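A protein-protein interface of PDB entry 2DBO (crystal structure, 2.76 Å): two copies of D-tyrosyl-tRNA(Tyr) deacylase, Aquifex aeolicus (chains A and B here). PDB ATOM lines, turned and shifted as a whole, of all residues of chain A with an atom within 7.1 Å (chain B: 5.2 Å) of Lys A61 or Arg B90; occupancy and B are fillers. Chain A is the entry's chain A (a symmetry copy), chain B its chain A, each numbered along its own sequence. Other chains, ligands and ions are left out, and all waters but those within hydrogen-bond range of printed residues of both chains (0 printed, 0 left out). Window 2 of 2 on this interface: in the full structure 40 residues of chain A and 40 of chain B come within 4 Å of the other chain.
Printed residues of chain A that touch a printed residue of chain B: Asn A51, Leu A52, Arg A53, Glu A56, Lys A61 and Phe A62. Hydrophobic or aromatic side chains of chain A within 4 Å of the printed part of chain B: Leu A52 and Phe A62. Among the printed residues, 10 pairs touch across the chains.
The backbone carbonyl oxygen (O) of Asn A51 lies close to the backbone carbonyl oxygen (O) of Arg B89. The side-chain sulfur (SD) of Met B128 sits close to the side-chain carboxylate (OE2) of Glu A56. The backbone NH (N) of Arg A53 is in hydrogen-bond range of the backbone carbonyl oxygen (O) of Arg B89 (2.9 Å).
No position is printed for both chains. Of the 10 pairs that touch across the chains among the printed residues, none has its exchanged pair printed and touching as well.
CA of Leu A52 touches O of Arg B89, at 3.5 Å. Leu A52 touches Pro B91 (CD2 to CD, 3.7 Å). N of Arg B90 touches CG of Arg A53, at 3.5 Å. CD of Pro B91 touches O of Arg A53 (3.5 Å). Arg B90 touches Lys A61 (NH2 to O, 3.6 Å). O of Phe A62 touches CD of Arg B90 (3.6 Å). Pro B91 touches Phe A62 (CG to CD1, 3.97 Å).
The side-chain carboxylate (OE2) of Glu A56 lies within salt-bridge range of the guanidinium group (NH1) of Arg A7, 2.9 Å away.
Arg A7 touches none of the printed residues of chain B. Printed residues of chain B within 4 Å of Leu A52: Arg B89 (3.5 Å) and Pro B91 (3.7 Å). Printed residues of chain B within 4 Å of Arg A53: Arg B89 (2.9 Å), Arg B90 (3.5 Å) and Pro B91 (3.5 Å). Of the printed residues of chain B, Glu A56 touches Met B128 (3.7 Å). Lys A61 touches just one residue of chain B: Arg B90. Of the printed residues of chain A, Arg B89 touches Asn A51, Leu A52 and Arg A53. Arg B90 touches just these residues of chain A: Arg A53 (3.5 Å), Lys A61 (3.6 Å) and Phe A62 (3.6 Å). Ser B92 touches none of the printed residues of chain A. Of the printed residues of chain A, Met B128 touches Glu A56 (3.7 Å). The nearest residue of chain B that does not touch Lys A61 is Met B128 (4.1 Å).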
ATOM      1  N   ARG A   7      19.972  -9.359 -25.130  1.00  0.00           N
ATOM      2  CA  ARG A   7      19.553 -10.514 -24.344  1.00  0.00           C
ATOM      3  C   ARG A   7      18.946 -11.492 -25.337  1.00  0.00           C
ATOM      4  O   ARG A   7      17.988 -11.159 -26.048  1.00  0.00           O
ATOM      5  CB  ARG A   7      18.502 -10.124 -23.295  1.00  0.00           C
ATOM      6  CG  ARG A   7      18.119 -11.279 -22.362  1.00  0.00           C
ATOM      7  CD  ARG A   7      17.092 -10.878 -21.296  1.00  0.00           C
ATOM      8  NE  ARG A   7      15.733 -10.792 -21.821  1.00  0.00           N
ATOM      9  CZ  ARG A   7      14.663 -10.471 -21.094  1.00  0.00           C
ATOM     10  NH1 ARG A   7      14.785 -10.200 -19.801  1.00  0.00           N
ATOM     11  NH2 ARG A   7      13.465 -10.429 -21.662  1.00  0.00           N
ATOM     12  N   ASN A  51      27.682  -8.074 -14.667  1.00  0.00           N
ATOM     13  CA  ASN A  51      26.787  -7.797 -13.542  1.00  0.00           C
ATOM     14  C   ASN A  51      25.493  -7.081 -13.921  1.00  0.00           C
ATOM     15  O   ASN A  51      24.739  -6.661 -13.045  1.00  0.00           O
ATOM     16  CB  ASN A  51      27.500  -6.958 -12.470  1.00  0.00           C
ATOM     17  CG  ASN A  51      28.840  -7.552 -12.036  1.00  0.00           C
ATOM     18  OD1 ASN A  51      28.955  -8.747 -11.739  1.00  0.00           O
ATOM     19  ND2 ASN A  51      29.861  -6.704 -11.981  1.00  0.00           N
ATOM     20  N   LEU A  52      25.224  -6.931 -15.209  1.00  0.00           N
ATOM     21  CA  LEU A  52      24.014  -6.235 -15.635  1.00  0.00           C
ATOM     22  C   LEU A  52      22.752  -7.029 -15.332  1.00  0.00           C
ATOM     23  O   LEU A  52      22.546  -8.117 -15.874  1.00  0.00           O
ATOM     24  CB  LEU A  52      24.074  -5.939 -17.133  1.00  0.00           C
ATOM     25  CG  LEU A  52      23.940  -4.482 -17.596  1.00  0.00           C
ATOM     26  CD1 LEU A  52      23.957  -4.490 -19.118  1.00  0.00           C
ATOM     27  CD2 LEU A  52      22.656  -3.822 -17.079  1.00  0.00           C
ATOM     28  N   ARG A  53      21.899  -6.480 -14.477  1.00  0.00           N
ATOM     29  CA  ARG A  53      20.662  -7.163 -14.132  1.00  0.00           C
ATOM     30  C   ARG A  53      19.624  -6.911 -15.223  1.00  0.00           C
ATOM     31  O   ARG A  53      18.787  -6.017 -15.086  1.00  0.00           O
ATOM     32  CB  ARG A  53      20.114  -6.661 -12.780  1.00  0.00           C
ATOM     33  CG  ARG A  53      21.179  -6.293 -11.748  1.00  0.00           C
ATOM     34  CD  ARG A  53      21.469  -7.387 -10.721  1.00  0.00           C
ATOM     35  NE  ARG A  53      21.098  -6.928  -9.382  1.00  0.00           N
ATOM     36  CZ  ARG A  53      21.653  -7.344  -8.245  1.00  0.00           C
ATOM     37  NH1 ARG A  53      22.634  -8.251  -8.253  1.00  0.00           N
ATOM     38  NH2 ARG A  53      21.224  -6.840  -7.097  1.00  0.00           N
ATOM     39  N   ILE A  54      19.679  -7.672 -16.314  1.00  0.00           N
ATOM     40  CA  ILE A  54      18.691  -7.502 -17.382  1.00  0.00           C
ATOM     41  C   ILE A  54      17.772  -8.712 -17.473  1.00  0.00           C
ATOM     42  O   ILE A  54      16.683  -8.635 -18.054  1.00  0.00           O
ATOM     43  CB  ILE A  54      19.329  -7.268 -18.774  1.00  0.00           C
ATOM     44  CG1 ILE A  54      20.320  -8.383 -19.098  1.00  0.00           C
ATOM     45  CG2 ILE A  54      19.956  -5.879 -18.828  1.00  0.00           C
ATOM     46  CD1 ILE A  54      20.749  -8.402 -20.557  1.00  0.00           C
ATOM     47  N   PHE A  55      18.206  -9.830 -16.895  1.00  0.00           N
ATOM     48  CA  PHE A  55      17.391 -11.040 -16.897  1.00  0.00           C
ATOM     49  C   PHE A  55      16.300 -10.940 -15.834  1.00  0.00           C
ATOM     50  O   PHE A  55      16.468 -10.264 -14.809  1.00  0.00           O
ATOM     51  CB  PHE A  55      18.257 -12.270 -16.659  1.00  0.00           C
ATOM     52  CG  PHE A  55      19.237 -12.515 -17.751  1.00  0.00           C
ATOM     53  CD1 PHE A  55      20.501 -11.927 -17.720  1.00  0.00           C
ATOM     54  CD2 PHE A  55      18.884 -13.297 -18.844  1.00  0.00           C
ATOM     55  CE1 PHE A  55      21.404 -12.119 -18.773  1.00  0.00           C
ATOM     56  CE2 PHE A  55      19.776 -13.500 -19.904  1.00  0.00           C
ATOM     57  CZ  PHE A  55      21.040 -12.911 -19.870  1.00  0.00           C
ATOM     58  N   GLU A  56      15.194 -11.629 -16.077  1.00  0.00           N
ATOM     59  CA  GLU A  56      14.042 -11.580 -15.188  1.00  0.00           C
ATOM     60  C   GLU A  56      13.430 -12.957 -14.934  1.00  0.00           C
ATOM     61  O   GLU A  56      13.745 -13.917 -15.634  1.00  0.00           O
ATOM     62  CB  GLU A  56      12.978 -10.722 -15.855  1.00  0.00           C
ATOM     63  CG  GLU A  56      12.567 -11.333 -17.194  1.00  0.00           C
ATOM     64  CD  GLU A  56      11.601 -10.488 -18.003  1.00  0.00           C
ATOM     65  OE1 GLU A  56      10.450 -10.266 -17.551  1.00  0.00           O
ATOM     66  OE2 GLU A  56      12.005 -10.052 -19.108  1.00  0.00           O
ATOM     67  N   ASP A  57      12.578 -13.053 -13.916  1.00  0.00           N
ATOM     68  CA  ASP A  57      11.843 -14.295 -13.682  1.00  0.00           C
ATOM     69  C   ASP A  57      10.391 -13.824 -13.707  1.00  0.00           C
ATOM     70  O   ASP A  57      10.110 -12.773 -14.290  1.00  0.00           O
ATOM     71  CB  ASP A  57      12.206 -15.011 -12.361  1.00  0.00           C
ATOM     72  CG  ASP A  57      12.055 -14.137 -11.131  1.00  0.00           C
ATOM     73  OD1 ASP A  57      11.135 -13.293 -11.096  1.00  0.00           O
ATOM     74  OD2 ASP A  57      12.853 -14.322 -10.179  1.00  0.00           O
ATOM     75  N   GLU A  58       9.469 -14.562 -13.099  1.00  0.00           N
ATOM     76  CA  GLU A  58       8.072 -14.137 -13.142  1.00  0.00           C
ATOM     77  C   GLU A  58       7.698 -13.113 -12.063  1.00  0.00           C
ATOM     78  O   GLU A  58       6.592 -12.563 -12.074  1.00  0.00           O
ATOM     79  CB  GLU A  58       7.143 -15.362 -13.059  1.00  0.00           C
ATOM     80  CG  GLU A  58       6.932 -15.978 -11.668  1.00  0.00           C
ATOM     81  CD  GLU A  58       8.200 -16.535 -11.027  1.00  0.00           C
ATOM     82  OE1 GLU A  58       9.169 -16.846 -11.751  1.00  0.00           O
ATOM     83  OE2 GLU A  58       8.217 -16.680  -9.784  1.00  0.00           O
ATOM     84  N   ARG A  59       8.638 -12.832 -11.166  1.00  0.00           N
ATOM     85  CA  ARG A  59       8.399 -11.906 -10.067  1.00  0.00           C
ATOM     86  C   ARG A  59       8.953 -10.491 -10.251  1.00  0.00           C
ATOM     87  O   ARG A  59       8.569  -9.563  -9.530  1.00  0.00           O
ATOM     88  CB  ARG A  59       8.946 -12.531  -8.778  1.00  0.00           C
ATOM     89  CG  ARG A  59       8.282 -13.871  -8.471  1.00  0.00           C
ATOM     90  CD  ARG A  59       9.153 -14.848  -7.688  1.00  0.00           C
ATOM     91  NE  ARG A  59       9.011 -14.723  -6.237  1.00  0.00           N
ATOM     92  CZ  ARG A  59       9.195 -15.728  -5.385  1.00  0.00           C
ATOM     93  NH1 ARG A  59       9.520 -16.935  -5.836  1.00  0.00           N
ATOM     94  NH2 ARG A  59       9.067 -15.521  -4.083  1.00  0.00           N
ATOM     95  N   GLY A  60       9.849 -10.310 -11.212  1.00  0.00           N
ATOM     96  CA  GLY A  60      10.408  -8.991 -11.433  1.00  0.00           C
ATOM     97  C   GLY A  60      11.384  -8.959 -12.585  1.00  0.00           C
ATOM     98  O   GLY A  60      12.136  -9.910 -12.806  1.00  0.00           O
ATOM     99  N   LYS A  61      11.365  -7.862 -13.331  1.00  0.00           N
ATOM    100  CA  LYS A  61      12.264  -7.682 -14.466  1.00  0.00           C
ATOM    101  C   LYS A  61      13.519  -6.959 -14.000  1.00  0.00           C
ATOM    102  O   LYS A  61      13.510  -6.278 -12.967  1.00  0.00           O
ATOM    103  CB  LYS A  61      11.576  -6.872 -15.566  1.00  0.00           C
ATOM    104  CG  LYS A  61      10.341  -7.556 -16.124  1.00  0.00           C
ATOM    105  CD  LYS A  61       9.679  -6.753 -17.232  1.00  0.00           C
ATOM    106  CE  LYS A  61       8.572  -7.582 -17.885  1.00  0.00           C
ATOM    107  NZ  LYS A  61       7.807  -6.850 -18.927  1.00  0.00           N
ATOM    108  N   PHE A  62      14.603  -7.120 -14.752  1.00  0.00           N
ATOM    109  CA  PHE A  62      15.862  -6.471 -14.417  1.00  0.00           C
ATOM    110  C   PHE A  62      16.324  -6.789 -13.001  1.00  0.00           C
ATOM    111  O   PHE A  62      16.472  -5.883 -12.178  1.00  0.00           O
ATOM    112  CB  PHE A  62      15.723  -4.948 -14.574  1.00  0.00           C
ATOM    113  CG  PHE A  62      15.274  -4.526 -15.938  1.00  0.00           C
ATOM    114  CD1 PHE A  62      16.131  -4.627 -17.029  1.00  0.00           C
ATOM    115  CD2 PHE A  62      13.982  -4.067 -16.147  1.00  0.00           C
ATOM    116  CE1 PHE A  62      15.702  -4.280 -18.313  1.00  0.00           C
ATOM    117  CE2 PHE A  62      13.543  -3.716 -17.423  1.00  0.00           C
ATOM    118  CZ  PHE A  62      14.409  -3.824 -18.510  1.00  0.00           C
ATOM    119  N   GLN A  63      16.532  -8.069 -12.704  1.00  0.00           N
ATOM    120  CA  GLN A  63      17.014  -8.442 -11.382  1.00  0.00           C
ATOM    121  C   GLN A  63      18.169  -9.431 -11.419  1.00  0.00           C
ATOM    122  O   GLN A  63      18.892  -9.567 -10.430  1.00  0.00           O
ATOM    123  CB  GLN A  63      15.869  -8.941 -10.474  1.00  0.00           C
ATOM    124  CG  GLN A  63      15.121 -10.194 -10.876  1.00  0.00           C
ATOM    125  CD  GLN A  63      14.121 -10.616  -9.796  1.00  0.00           C
ATOM    126  OE1 GLN A  63      14.504 -10.982  -8.682  1.00  0.00           O
ATOM    127  NE2 GLN A  63      12.834 -10.554 -10.122  1.00  0.00           N
ATOM    128  N   TYR A  64      18.379 -10.092 -12.557  1.00  0.00           N
ATOM    129  CA  TYR A  64      19.492 -11.034 -12.673  1.00  0.00           C
ATOM    130  C   TYR A  64      20.492 -10.709 -13.781  1.00  0.00           C
ATOM    131  O   TYR A  64      20.125 -10.272 -14.872  1.00  0.00           O
ATOM    132  CB  TYR A  64      18.992 -12.457 -12.896  1.00  0.00           C
ATOM    133  CG  TYR A  64      18.006 -12.922 -11.870  1.00  0.00           C
ATOM    134  CD1 TYR A  64      16.655 -13.047 -12.186  1.00  0.00           C
ATOM    135  CD2 TYR A  64      18.409 -13.221 -10.570  1.00  0.00           C
ATOM    136  CE1 TYR A  64      15.727 -13.462 -11.237  1.00  0.00           C
ATOM    137  CE2 TYR A  64      17.487 -13.637  -9.608  1.00  0.00           C
ATOM    138  CZ  TYR A  64      16.148 -13.755  -9.952  1.00  0.00           C
ATOM    139  OH  TYR A  64      15.228 -14.178  -9.017  1.00  0.00           O
ATOM    140  N   ASN B  84      20.832   3.432 -18.406  1.00  0.00           N
ATOM    141  CA  ASN B  84      21.933   4.026 -17.683  1.00  0.00           C
ATOM    142  C   ASN B  84      22.505   2.916 -16.819  1.00  0.00           C
ATOM    143  O   ASN B  84      21.818   2.400 -15.938  1.00  0.00           O
ATOM    144  CB  ASN B  84      21.414   5.155 -16.799  1.00  0.00           C
ATOM    145  CG  ASN B  84      22.528   5.965 -16.168  1.00  0.00           C
ATOM    146  OD1 ASN B  84      23.619   5.450 -15.895  1.00  0.00           O
ATOM    147  ND2 ASN B  84      22.251   7.241 -15.913  1.00  0.00           N
ATOM    148  N   LYS B  87      25.627   3.408 -12.498  1.00  0.00           N
ATOM    149  CA  LYS B  87      25.786   3.073 -11.089  1.00  0.00           C
ATOM    150  C   LYS B  87      25.614   1.603 -10.725  1.00  0.00           C
ATOM    151  O   LYS B  87      26.548   0.812 -10.867  1.00  0.00           O
ATOM    152  CB  LYS B  87      24.866   3.923 -10.202  1.00  0.00           C
ATOM    153  CG  LYS B  87      23.886   4.829 -10.910  1.00  0.00           C
ATOM    154  CD  LYS B  87      22.855   4.041 -11.694  1.00  0.00           C
ATOM    155  CE  LYS B  87      21.520   4.781 -11.746  1.00  0.00           C
ATOM    156  NZ  LYS B  87      21.629   6.191 -12.214  1.00  0.00           N
ATOM    157  N   GLY B  88      24.422   1.240 -10.259  1.00  0.00           N
ATOM    158  CA  GLY B  88      24.184  -0.129  -9.845  1.00  0.00           C
ATOM    159  C   GLY B  88      24.293  -1.221 -10.891  1.00  0.00           C
ATOM    160  O   GLY B  88      24.574  -0.962 -12.068  1.00  0.00           O
ATOM    161  N   ARG B  89      24.088  -2.456 -10.435  1.00  0.00           N
ATOM    162  CA  ARG B  89      24.101  -3.620 -11.305  1.00  0.00           C
ATOM    163  C   ARG B  89      22.826  -3.503 -12.147  1.00  0.00           C
ATOM    164  O   ARG B  89      22.771  -3.964 -13.295  1.00  0.00           O
ATOM    165  CB  ARG B  89      24.070  -4.902 -10.471  1.00  0.00           C
ATOM    166  CG  ARG B  89      25.325  -5.133  -9.646  1.00  0.00           C
ATOM    167  CD  ARG B  89      25.164  -6.316  -8.702  1.00  0.00           C
ATOM    168  NE  ARG B  89      26.443  -6.940  -8.364  1.00  0.00           N
ATOM    169  CZ  ARG B  89      26.568  -8.028  -7.608  1.00  0.00           C
ATOM    170  NH1 ARG B  89      25.490  -8.617  -7.102  1.00  0.00           N
ATOM    171  NH2 ARG B  89      27.768  -8.543  -7.369  1.00  0.00           N
ATOM    172  N   ARG B  90      21.806  -2.873 -11.563  1.00  0.00           N
ATOM    173  CA  ARG B  90      20.540  -2.662 -12.250  1.00  0.00           C
ATOM    174  C   ARG B  90      20.569  -1.374 -13.069  1.00  0.00           C
ATOM    175  O   ARG B  90      20.964  -0.314 -12.579  1.00  0.00           O
ATOM    176  CB  ARG B  90      19.369  -2.599 -11.265  1.00  0.00           C
ATOM    177  CG  ARG B  90      18.118  -2.056 -11.936  1.00  0.00           C
ATOM    178  CD  ARG B  90      16.809  -2.400 -11.244  1.00  0.00           C
ATOM    179  NE  ARG B  90      15.694  -1.851 -12.019  1.00  0.00           N
ATOM    180  CZ  ARG B  90      14.433  -2.274 -11.952  1.00  0.00           C
ATOM    181  NH1 ARG B  90      13.507  -1.694 -12.713  1.00  0.00           N
ATOM    182  NH2 ARG B  90      14.097  -3.273 -11.137  1.00  0.00           N
ATOM    183  N   PRO B  91      20.141  -1.452 -14.336  1.00  0.00           N
ATOM    184  CA  PRO B  91      20.123  -0.287 -15.223  1.00  0.00           C
ATOM    185  C   PRO B  91      18.999   0.690 -14.925  1.00  0.00           C
ATOM    186  O   PRO B  91      17.919   0.290 -14.490  1.00  0.00           O
ATOM    187  CB  PRO B  91      19.979  -0.916 -16.601  1.00  0.00           C
ATOM    188  CG  PRO B  91      19.120  -2.122 -16.310  1.00  0.00           C
ATOM    189  CD  PRO B  91      19.762  -2.679 -15.065  1.00  0.00           C
ATOM    190  N   SER B  92      19.262   1.970 -15.181  1.00  0.00           N
ATOM    191  CA  SER B  92      18.287   3.034 -14.968  1.00  0.00           C
ATOM    192  C   SER B  92      17.734   3.498 -16.318  1.00  0.00           C
ATOM    193  O   SER B  92      18.375   3.298 -17.347  1.00  0.00           O
ATOM    194  CB  SER B  92      18.958   4.208 -14.255  1.00  0.00           C
ATOM    195  OG  SER B  92      18.214   5.400 -14.448  1.00  0.00           O
ATOM    196  N   MET B 128       5.910  -7.719 -24.336  1.00  0.00           N
ATOM    197  CA  MET B 128       7.081  -8.490 -24.739  1.00  0.00           C
ATOM    198  C   MET B 128       6.980  -9.208 -26.079  1.00  0.00           C
ATOM    199  O   MET B 128       5.918  -9.688 -26.470  1.00  0.00           O
ATOM    200  CB  MET B 128       7.454  -9.489 -23.649  1.00  0.00           C
ATOM    201  CG  MET B 128       8.108  -8.838 -22.447  1.00  0.00           C
ATOM    202  SD  MET B 128       9.263  -9.958 -21.599  1.00  0.00           S
ATOM    203  CE  MET B 128       8.103 -10.772 -20.400  1.00  0.00           C
